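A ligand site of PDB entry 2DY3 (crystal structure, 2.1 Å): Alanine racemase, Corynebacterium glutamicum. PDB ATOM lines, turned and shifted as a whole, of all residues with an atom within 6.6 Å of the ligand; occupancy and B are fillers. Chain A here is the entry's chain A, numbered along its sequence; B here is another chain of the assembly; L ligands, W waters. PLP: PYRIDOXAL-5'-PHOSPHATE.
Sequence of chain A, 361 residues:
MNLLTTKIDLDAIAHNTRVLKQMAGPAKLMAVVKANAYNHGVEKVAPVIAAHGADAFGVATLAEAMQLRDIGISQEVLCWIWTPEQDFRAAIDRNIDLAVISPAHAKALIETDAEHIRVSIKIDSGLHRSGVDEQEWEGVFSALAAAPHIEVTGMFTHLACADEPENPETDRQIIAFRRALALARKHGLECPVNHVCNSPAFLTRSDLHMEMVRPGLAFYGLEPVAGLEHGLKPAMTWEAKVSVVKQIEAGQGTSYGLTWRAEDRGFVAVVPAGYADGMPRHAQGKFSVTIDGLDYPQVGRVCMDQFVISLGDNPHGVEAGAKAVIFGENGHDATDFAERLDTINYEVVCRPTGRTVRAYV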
ATOM      1  N   VAL A  32     -12.367  22.268 -21.198  1.00  0.00           N
ATOM      2  CA  VAL A  32     -13.646  22.849 -20.814  1.00  0.00           C
ATOM      3  C   VAL A  32     -13.724  24.237 -21.427  1.00  0.00           C
ATOM      4  O   VAL A  32     -12.918  25.096 -21.109  1.00  0.00           O
ATOM      5  CB  VAL A  32     -13.798  22.944 -19.278  1.00  0.00           C
ATOM      6  CG1 VAL A  32     -15.199  23.472 -18.916  1.00  0.00           C
ATOM      7  CG2 VAL A  32     -13.565  21.585 -18.639  1.00  0.00           C
ATOM      8  N   LYS A  34     -16.896  25.954 -21.720  1.00  0.00           N
ATOM      9  CA  LYS A  34     -18.236  26.448 -21.421  1.00  0.00           C
ATOM     10  C   LYS A  34     -18.148  27.970 -21.241  1.00  0.00           C
ATOM     11  O   LYS A  34     -17.056  28.528 -21.184  1.00  0.00           O
ATOM     12  CB  LYS A  34     -18.743  25.787 -20.133  1.00  0.00           C
ATOM     13  CG  LYS A  34     -17.927  26.199 -18.920  1.00  0.00           C
ATOM     14  CD  LYS A  34     -18.056  25.226 -17.749  1.00  0.00           C
ATOM     15  CE  LYS A  34     -17.669  25.973 -16.503  1.00  0.00           C
ATOM     16  NZ  LYS A  34     -17.115  25.291 -15.302  1.00  0.00           N
ATOM     17  N   TYR A  38     -14.910  30.567 -21.351  1.00  0.00           N
ATOM     18  CA  TYR A  38     -14.597  31.474 -20.256  1.00  0.00           C
ATOM     19  C   TYR A  38     -14.468  32.898 -20.774  1.00  0.00           C
ATOM     20  O   TYR A  38     -13.532  33.625 -20.439  1.00  0.00           O
ATOM     21  CB  TYR A  38     -13.295  31.042 -19.569  1.00  0.00           C
ATOM     22  CG  TYR A  38     -13.424  29.796 -18.691  1.00  0.00           C
ATOM     23  CD1 TYR A  38     -14.134  28.678 -19.142  1.00  0.00           C
ATOM     24  CD2 TYR A  38     -12.805  29.730 -17.445  1.00  0.00           C
ATOM     25  CE1 TYR A  38     -14.226  27.524 -18.362  1.00  0.00           C
ATOM     26  CE2 TYR A  38     -12.888  28.571 -16.667  1.00  0.00           C
ATOM     27  CZ  TYR A  38     -13.593  27.470 -17.132  1.00  0.00           C
ATOM     28  OH  TYR A  38     -13.679  26.332 -16.367  1.00  0.00           O
ATOM     29  N   ALA A  60     -21.233  23.244 -20.508  1.00  0.00           N
ATOM     30  CA  ALA A  60     -22.352  23.075 -19.600  1.00  0.00           C
ATOM     31  C   ALA A  60     -23.661  22.742 -20.293  1.00  0.00           C
ATOM     32  O   ALA A  60     -24.268  21.719 -19.990  1.00  0.00           O
ATOM     33  CB  ALA A  60     -22.529  24.340 -18.732  1.00  0.00           C
ATOM     34  N   TRP A  80     -23.123  18.725 -19.524  1.00  0.00           N
ATOM     35  CA  TRP A  80     -23.625  18.277 -18.228  1.00  0.00           C
ATOM     36  C   TRP A  80     -24.744  19.063 -17.542  1.00  0.00           C
ATOM     37  O   TRP A  80     -25.142  18.711 -16.425  1.00  0.00           O
ATOM     38  CB  TRP A  80     -22.447  18.101 -17.264  1.00  0.00           C
ATOM     39  CG  TRP A  80     -21.542  19.301 -17.183  1.00  0.00           C
ATOM     40  CD1 TRP A  80     -21.799  20.471 -16.539  1.00  0.00           C
ATOM     41  CD2 TRP A  80     -20.241  19.434 -17.767  1.00  0.00           C
ATOM     42  NE1 TRP A  80     -20.733  21.326 -16.679  1.00  0.00           N
ATOM     43  CE2 TRP A  80     -19.768  20.714 -17.434  1.00  0.00           C
ATOM     44  CE3 TRP A  80     -19.428  18.591 -18.539  1.00  0.00           C
ATOM     45  CZ2 TRP A  80     -18.517  21.178 -17.835  1.00  0.00           C
ATOM     46  CZ3 TRP A  80     -18.186  19.059 -18.939  1.00  0.00           C
ATOM     47  CH2 TRP A  80     -17.744  20.336 -18.586  1.00  0.00           C
ATOM     48  N   ILE A  81     -25.241  20.113 -18.167  1.00  0.00           N
ATOM     49  CA  ILE A  81     -26.332  20.852 -17.565  1.00  0.00           C
ATOM     50  C   ILE A  81     -27.480  20.962 -18.558  1.00  0.00           C
ATOM     51  O   ILE A  81     -27.474  21.823 -19.437  1.00  0.00           O
ATOM     52  CB  ILE A  81     -25.889  22.278 -17.120  1.00  0.00           C
ATOM     53  CG1 ILE A  81     -24.835  22.169 -16.028  1.00  0.00           C
ATOM     54  CG2 ILE A  81     -27.087  23.050 -16.568  1.00  0.00           C
ATOM     55  CD1 ILE A  81     -24.416  23.510 -15.438  1.00  0.00           C
ATOM     56  N   LYS A 122     -22.859  11.475 -13.977  1.00  0.00           N
ATOM     57  CA  LYS A 122     -22.346  12.498 -13.081  1.00  0.00           C
ATOM     58  C   LYS A 122     -22.622  12.005 -11.672  1.00  0.00           C
ATOM     59  O   LYS A 122     -23.776  11.810 -11.286  1.00  0.00           O
ATOM     60  CB  LYS A 122     -23.041  13.837 -13.308  1.00  0.00           C
ATOM     61  CG  LYS A 122     -22.400  14.991 -12.551  1.00  0.00           C
ATOM     62  CD  LYS A 122     -23.157  16.292 -12.767  1.00  0.00           C
ATOM     63  CE  LYS A 122     -22.549  17.422 -11.944  1.00  0.00           C
ATOM     64  NZ  LYS A 122     -21.262  17.900 -12.484  1.00  0.00           N
ATOM     65  N   PHE A 156     -18.048  10.597 -13.862  1.00  0.00           N
ATOM     66  CA  PHE A 156     -17.220  11.705 -13.421  1.00  0.00           C
ATOM     67  C   PHE A 156     -17.858  12.423 -12.248  1.00  0.00           C
ATOM     68  O   PHE A 156     -19.047  12.277 -11.985  1.00  0.00           O
ATOM     69  CB  PHE A 156     -16.997  12.692 -14.557  1.00  0.00           C
ATOM     70  CG  PHE A 156     -18.266  13.382 -15.031  1.00  0.00           C
ATOM     71  CD1 PHE A 156     -19.235  12.691 -15.739  1.00  0.00           C
ATOM     72  CD2 PHE A 156     -18.464  14.734 -14.777  1.00  0.00           C
ATOM     73  CE1 PHE A 156     -20.385  13.336 -16.186  1.00  0.00           C
ATOM     74  CE2 PHE A 156     -19.611  15.381 -15.215  1.00  0.00           C
ATOM     75  CZ  PHE A 156     -20.571  14.685 -15.925  1.00  0.00           C
ATOM     76  N   THR A 157     -17.053  13.190 -11.527  1.00  0.00           N
ATOM     77  CA  THR A 157     -17.545  13.968 -10.392  1.00  0.00           C
ATOM     78  C   THR A 157     -16.699  15.249 -10.360  1.00  0.00           C
ATOM     79  O   THR A 157     -15.680  15.333 -11.038  1.00  0.00           O
ATOM     80  CB  THR A 157     -17.366  13.192  -9.074  1.00  0.00           C
ATOM     81  OG1 THR A 157     -18.185  13.790  -8.053  1.00  0.00           O
ATOM     82  CG2 THR A 157     -15.916  13.224  -8.635  1.00  0.00           C
ATOM     83  N   HIS A 158     -17.138  16.231  -9.586  1.00  0.00           N
ATOM     84  CA  HIS A 158     -16.408  17.494  -9.519  1.00  0.00           C
ATOM     85  C   HIS A 158     -15.900  17.773  -8.097  1.00  0.00           C
ATOM     86  O   HIS A 158     -16.657  17.696  -7.135  1.00  0.00           O
ATOM     87  CB  HIS A 158     -17.324  18.623 -10.000  1.00  0.00           C
ATOM     88  CG  HIS A 158     -16.608  19.872 -10.378  1.00  0.00           C
ATOM     89  ND1 HIS A 158     -15.454  19.873 -11.142  1.00  0.00           N
ATOM     90  CD2 HIS A 158     -16.885  21.179 -10.127  1.00  0.00           C
ATOM     91  CE1 HIS A 158     -15.062  21.109 -11.346  1.00  0.00           C
ATOM     92  NE2 HIS A 158     -15.911  21.922 -10.738  1.00  0.00           N
ATOM     93  N   CYS A 197     -10.483  15.277 -12.601  1.00  0.00           N
ATOM     94  CA  CYS A 197      -9.577  16.423 -12.554  1.00  0.00           C
ATOM     95  C   CYS A 197      -9.937  17.673 -13.341  1.00  0.00           C
ATOM     96  O   CYS A 197     -10.086  17.650 -14.565  1.00  0.00           O
ATOM     97  CB  CYS A 197      -8.156  16.004 -12.981  1.00  0.00           C
ATOM     98  SG  CYS A 197      -7.243  15.034 -11.759  1.00  0.00           S
ATOM     99  N   ASN A 198     -10.084  18.776 -12.602  1.00  0.00           N
ATOM    100  CA  ASN A 198     -10.337  20.077 -13.196  1.00  0.00           C
ATOM    101  C   ASN A 198      -8.917  20.633 -13.197  1.00  0.00           C
ATOM    102  O   ASN A 198      -7.982  19.886 -12.895  1.00  0.00           O
ATOM    103  CB  ASN A 198     -11.225  20.923 -12.289  1.00  0.00           C
ATOM    104  CG  ASN A 198     -10.744  20.937 -10.850  1.00  0.00           C
ATOM    105  OD1 ASN A 198      -9.709  20.357 -10.518  1.00  0.00           O
ATOM    106  ND2 ASN A 198     -11.494  21.597  -9.983  1.00  0.00           N
ATOM    107  N   SER A 199      -8.737  21.914 -13.497  1.00  0.00           N
ATOM    108  CA  SER A 199      -7.393  22.499 -13.555  1.00  0.00           C
ATOM    109  C   SER A 199      -6.499  22.308 -12.323  1.00  0.00           C
ATOM    110  O   SER A 199      -5.378  21.825 -12.438  1.00  0.00           O
ATOM    111  CB  SER A 199      -7.472  23.984 -13.900  1.00  0.00           C
ATOM    112  OG  SER A 199      -7.815  24.175 -15.271  1.00  0.00           O
ATOM    113  N   PRO A 200      -6.990  22.674 -11.124  1.00  0.00           N
ATOM    114  CA  PRO A 200      -6.153  22.497  -9.931  1.00  0.00           C
ATOM    115  C   PRO A 200      -5.748  21.057  -9.598  1.00  0.00           C
ATOM    116  O   PRO A 200      -4.582  20.796  -9.288  1.00  0.00           O
ATOM    117  CB  PRO A 200      -6.969  23.154  -8.815  1.00  0.00           C
ATOM    118  CG  PRO A 200      -8.379  23.050  -9.327  1.00  0.00           C
ATOM    119  CD  PRO A 200      -8.239  23.378 -10.778  1.00  0.00           C
ATOM    120  N   ARG A 214     -10.123  16.929 -17.042  1.00  0.00           N
ATOM    121  CA  ARG A 214     -11.062  17.970 -17.471  1.00  0.00           C
ATOM    122  C   ARG A 214     -10.665  19.405 -17.110  1.00  0.00           C
ATOM    123  O   ARG A 214     -11.355  20.059 -16.332  1.00  0.00           O
ATOM    124  CB  ARG A 214     -12.427  17.642 -16.840  1.00  0.00           C
ATOM    125  CG  ARG A 214     -13.640  18.293 -17.449  1.00  0.00           C
ATOM    126  CD  ARG A 214     -14.846  18.046 -16.558  1.00  0.00           C
ATOM    127  NE  ARG A 214     -14.769  16.726 -15.945  1.00  0.00           N
ATOM    128  CZ  ARG A 214     -14.786  16.496 -14.637  1.00  0.00           C
ATOM    129  NH1 ARG A 214     -14.891  17.500 -13.779  1.00  0.00           N
ATOM    130  NH2 ARG A 214     -14.690  15.257 -14.188  1.00  0.00           N
ATOM    131  N   PRO A 215      -9.573  19.913 -17.685  1.00  0.00           N
ATOM    132  CA  PRO A 215      -9.147  21.282 -17.353  1.00  0.00           C
ATOM    133  C   PRO A 215      -9.852  22.390 -18.150  1.00  0.00           C
ATOM    134  O   PRO A 215     -10.126  22.239 -19.341  1.00  0.00           O
ATOM    135  CB  PRO A 215      -7.642  21.263 -17.666  1.00  0.00           C
ATOM    136  CG  PRO A 215      -7.309  19.782 -17.883  1.00  0.00           C
ATOM    137  CD  PRO A 215      -8.543  19.247 -18.491  1.00  0.00           C
ATOM    138  N   GLY A 216     -10.137  23.484 -17.456  1.00  0.00           N
ATOM    139  CA  GLY A 216     -10.766  24.636 -18.092  1.00  0.00           C
ATOM    140  C   GLY A 216      -9.820  25.825 -17.947  1.00  0.00           C
ATOM    141  O   GLY A 216      -9.117  26.200 -18.898  1.00  0.00           O
ATOM    142  N   LEU A 217      -9.786  26.378 -16.742  1.00  0.00           N
ATOM    143  CA  LEU A 217      -8.952  27.529 -16.382  1.00  0.00           C
ATOM    144  C   LEU A 217      -7.558  27.580 -17.032  1.00  0.00           C
ATOM    145  O   LEU A 217      -7.189  28.573 -17.663  1.00  0.00           O
ATOM    146  CB  LEU A 217      -8.769  27.551 -14.864  1.00  0.00           C
ATOM    147  CG  LEU A 217      -8.611  28.887 -14.139  1.00  0.00           C
ATOM    148  CD1 LEU A 217      -7.409  28.839 -13.201  1.00  0.00           C
ATOM    149  CD2 LEU A 217      -8.461  29.997 -15.148  1.00  0.00           C
ATOM    150  N   ALA A 218      -6.783  26.510 -16.846  1.00  0.00           N
ATOM    151  CA  ALA A 218      -5.417  26.429 -17.363  1.00  0.00           C
ATOM    152  C   ALA A 218      -5.231  26.750 -18.847  1.00  0.00           C
ATOM    153  O   ALA A 218      -4.215  27.347 -19.226  1.00  0.00           O
ATOM    154  CB  ALA A 218      -4.830  25.063 -17.039  1.00  0.00           C
ATOM    155  N   TYR A 220      -6.558  28.909 -20.507  1.00  0.00           N
ATOM    156  CA  TYR A 220      -6.559  30.349 -20.688  1.00  0.00           C
ATOM    157  C   TYR A 220      -5.345  30.978 -20.015  1.00  0.00           C
ATOM    158  O   TYR A 220      -5.261  32.200 -19.903  1.00  0.00           O
ATOM    159  CB  TYR A 220      -7.870  30.920 -20.147  1.00  0.00           C
ATOM    160  CG  TYR A 220      -9.056  30.150 -20.669  1.00  0.00           C
ATOM    161  CD1 TYR A 220      -9.446  30.251 -21.993  1.00  0.00           C
ATOM    162  CD2 TYR A 220      -9.735  29.257 -19.843  1.00  0.00           C
ATOM    163  CE1 TYR A 220     -10.474  29.474 -22.494  1.00  0.00           C
ATOM    164  CE2 TYR A 220     -10.766  28.471 -20.341  1.00  0.00           C
ATOM    165  CZ  TYR A 220     -11.137  28.587 -21.663  1.00  0.00           C
ATOM    166  OH  TYR A 220     -12.146  27.801 -22.167  1.00  0.00           O
ATOM    167  N   PRO A 224      -4.585  27.947 -11.045  1.00  0.00           N
ATOM    168  CA  PRO A 224      -5.615  27.688 -10.033  1.00  0.00           C
ATOM    169  C   PRO A 224      -5.079  27.730  -8.613  1.00  0.00           C
ATOM    170  O   PRO A 224      -5.725  28.241  -7.710  1.00  0.00           O
ATOM    171  CB  PRO A 224      -6.101  26.281 -10.395  1.00  0.00           C
ATOM    172  CG  PRO A 224      -5.751  26.143 -11.852  1.00  0.00           C
ATOM    173  CD  PRO A 224      -4.394  26.778 -11.911  1.00  0.00           C
ATOM    174  N   TYR A 346     -11.294  33.160 -12.100  1.00  0.00           N
ATOM    175  CA  TYR A 346     -12.351  32.595 -12.941  1.00  0.00           C
ATOM    176  C   TYR A 346     -13.406  33.643 -13.287  1.00  0.00           C
ATOM    177  O   TYR A 346     -13.876  33.717 -14.429  1.00  0.00           O
ATOM    178  CB  TYR A 346     -13.082  31.457 -12.230  1.00  0.00           C
ATOM    179  CG  TYR A 346     -12.295  30.197 -12.019  1.00  0.00           C
ATOM    180  CD1 TYR A 346     -11.354  30.095 -11.002  1.00  0.00           C
ATOM    181  CD2 TYR A 346     -12.509  29.078 -12.825  1.00  0.00           C
ATOM    182  CE1 TYR A 346     -10.656  28.923 -10.780  1.00  0.00           C
ATOM    183  CE2 TYR A 346     -11.814  27.905 -12.612  1.00  0.00           C
ATOM    184  CZ  TYR A 346     -10.892  27.833 -11.595  1.00  0.00           C
ATOM    185  OH  TYR A 346     -10.188  26.655 -11.384  1.00  0.00           O
ATOM    186  N   MET B 304     -19.500  28.883 -11.164  1.00  0.00           N
ATOM    187  CA  MET B 304     -19.490  29.471 -12.494  1.00  0.00           C
ATOM    188  C   MET B 304     -20.785  29.290 -13.266  1.00  0.00           C
ATOM    189  O   MET B 304     -21.269  30.216 -13.917  1.00  0.00           O
ATOM    190  CB  MET B 304     -18.316  28.918 -13.315  1.00  0.00           C
ATOM    191  CG  MET B 304     -17.968  29.775 -14.517  1.00  0.00           C
ATOM    192  SD  MET B 304     -16.395  29.368 -15.354  1.00  0.00           S
ATOM    193  CE  MET B 304     -16.903  29.550 -17.025  1.00  0.00           C
ATOM    194  N   ASP B 305     -21.370  28.097 -13.174  1.00  0.00           N
ATOM    195  CA  ASP B 305     -22.591  27.831 -13.932  1.00  0.00           C
ATOM    196  C   ASP B 305     -23.865  27.676 -13.100  1.00  0.00           C
ATOM    197  O   ASP B 305     -24.951  27.561 -13.667  1.00  0.00           O
ATOM    198  CB  ASP B 305     -22.407  26.563 -14.760  1.00  0.00           C
ATOM    199  CG  ASP B 305     -21.099  26.553 -15.523  1.00  0.00           C
ATOM    200  OD1 ASP B 305     -20.895  27.442 -16.387  1.00  0.00           O
ATOM    201  OD2 ASP B 305     -20.281  25.654 -15.261  1.00  0.00           O
HETATM  202  N1  PLP L   1     -15.557  20.283 -14.856  1.00  0.00           N
HETATM  203  C2  PLP L   1     -16.844  20.788 -14.720  1.00  0.00           C
HETATM  204  C2A PLP L   1     -18.004  19.829 -14.455  1.00  0.00           C
HETATM  205  C3  PLP L   1     -17.044  22.188 -14.830  1.00  0.00           C
HETATM  206  O3  PLP L   1     -18.320  22.712 -14.690  1.00  0.00           O
HETATM  207  C4  PLP L   1     -15.936  23.037 -15.085  1.00  0.00           C
HETATM  208  C4A PLP L   1     -16.056  24.582 -15.155  1.00  0.00           C
HETATM  209  C5  PLP L   1     -14.614  22.455 -15.198  1.00  0.00           C
HETATM  210  C6  PLP L   1     -14.455  21.086 -15.081  1.00  0.00           C
HETATM  211  C5A PLP L   1     -13.388  23.282 -15.429  1.00  0.00           C
HETATM  212  O4P PLP L   1     -12.755  23.620 -14.207  1.00  0.00           O
HETATM  213  P   PLP L   1     -11.409  24.505 -14.030  1.00  0.00           P
HETATM  214  O1P PLP L   1     -11.556  25.761 -14.782  1.00  0.00           O
HETATM  215  O2P PLP L   1     -11.379  24.707 -12.592  1.00  0.00           O
HETATM  216  O3P PLP L   1     -10.369  23.622 -14.585  1.00  0.00           O
HETATM  217  O   HOH W   1     -21.107  23.131 -14.530  1.00  0.00           O
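CG2 of Val 32 touches C5A of the ligand, at 3.6 Å.
CE1 of His 158 touches N1 of the ligand, at 3.6 Å.
C of Asn 198 touches O3P of the ligand, 3.6 Å away.
CD of Pro 200 touches O2P of the ligand, at 3.9 Å.
C of Pro 215 touches O3P of the ligand, at 3.8 Å.
Asp 305 of chain B touches the ligand (OD2 to O3, 3.6 Å).
14 residues have an atom within 4 Å of the ligand: Val 32, Lys 34, Tyr 38, Trp 80, His 158, Asn 198, Ser 199, Pro 200, Arg 214, Pro 215, Gly 216, Leu 217, Tyr 346 and Asp 305 of chain B.
The nearest printed residue that does not touch the ligand is Lys 122 (4.3 Å).
Water W1 lies within hydrogen-bond range of OD2 of Asp 305 of chain B (2.8 Å), O3 of the ligand (2.8 Å) and NE1 of Trp 80 (2.8 Å).
The backbone NH (N) of Leu 217 is in hydrogen-bond range of an oxygen (O1P) of the ligand (2.7 Å).
O2P of the ligand lies within hydrogen-bond range of OH of Tyr 346, at 2.6 Å.
The indole nitrogen (NE1) of Trp 80 sits at hydrogen-bond distance from an oxygen (O3) of the ligand.
N of Gly 216 lies within hydrogen-bond range of O3P of the ligand (2.9 Å).
A carbon (C4A) of the ligand is covalently linked to the side-chain amino group of Lys 34 (1.3 Å).
The guanidinium group (NH1) of Arg 214 lies close to a nitrogen (N1) of the ligand, 3.1 Å away.
N of Ser 199 is in hydrogen-bond range of O3P of the ligand (2.6 Å).
O3P of the ligand sits at hydrogen-bond distance from OG of Ser 199, at 2.7 Å.
An oxygen (O1P) of the ligand sits at hydrogen-bond distance from the side-chain hydroxyl (OH) of Tyr 38 (2.7 Å).
OH of Tyr 220 is in hydrogen-bond range of O of Val 32 (3.0 Å).
The side-chain hydroxyl (OG) of Ser 199 sits at hydrogen-bond distance from the backbone NH (N) of Leu 217 (3.3 Å).
N of Val 32 lies within hydrogen-bond range of O of Pro 215, 2.9 Å away.
The guanidinium group (NH2) of Arg 214 sits at hydrogen-bond distance from the backbone carbonyl oxygen (O) of Thr 157, at 3.3 Å.
The backbone carbonyl oxygen (O) of Ala 60 is in hydrogen-bond range of the backbone NH (N) of Trp 80.
The backbone carbonyl oxygen (O) of Cys 197 sits at hydrogen-bond distance from the backbone NH (N) of Arg 214, 2.6 Å away.
N of Ala 218 is in hydrogen-bond range of OG of Ser 199, 3.0 Å away.
The side-chain amino group of Lys 34 lies within salt-bridge range of the side-chain carboxylate of Asp 305 of chain B (3.2 Å).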
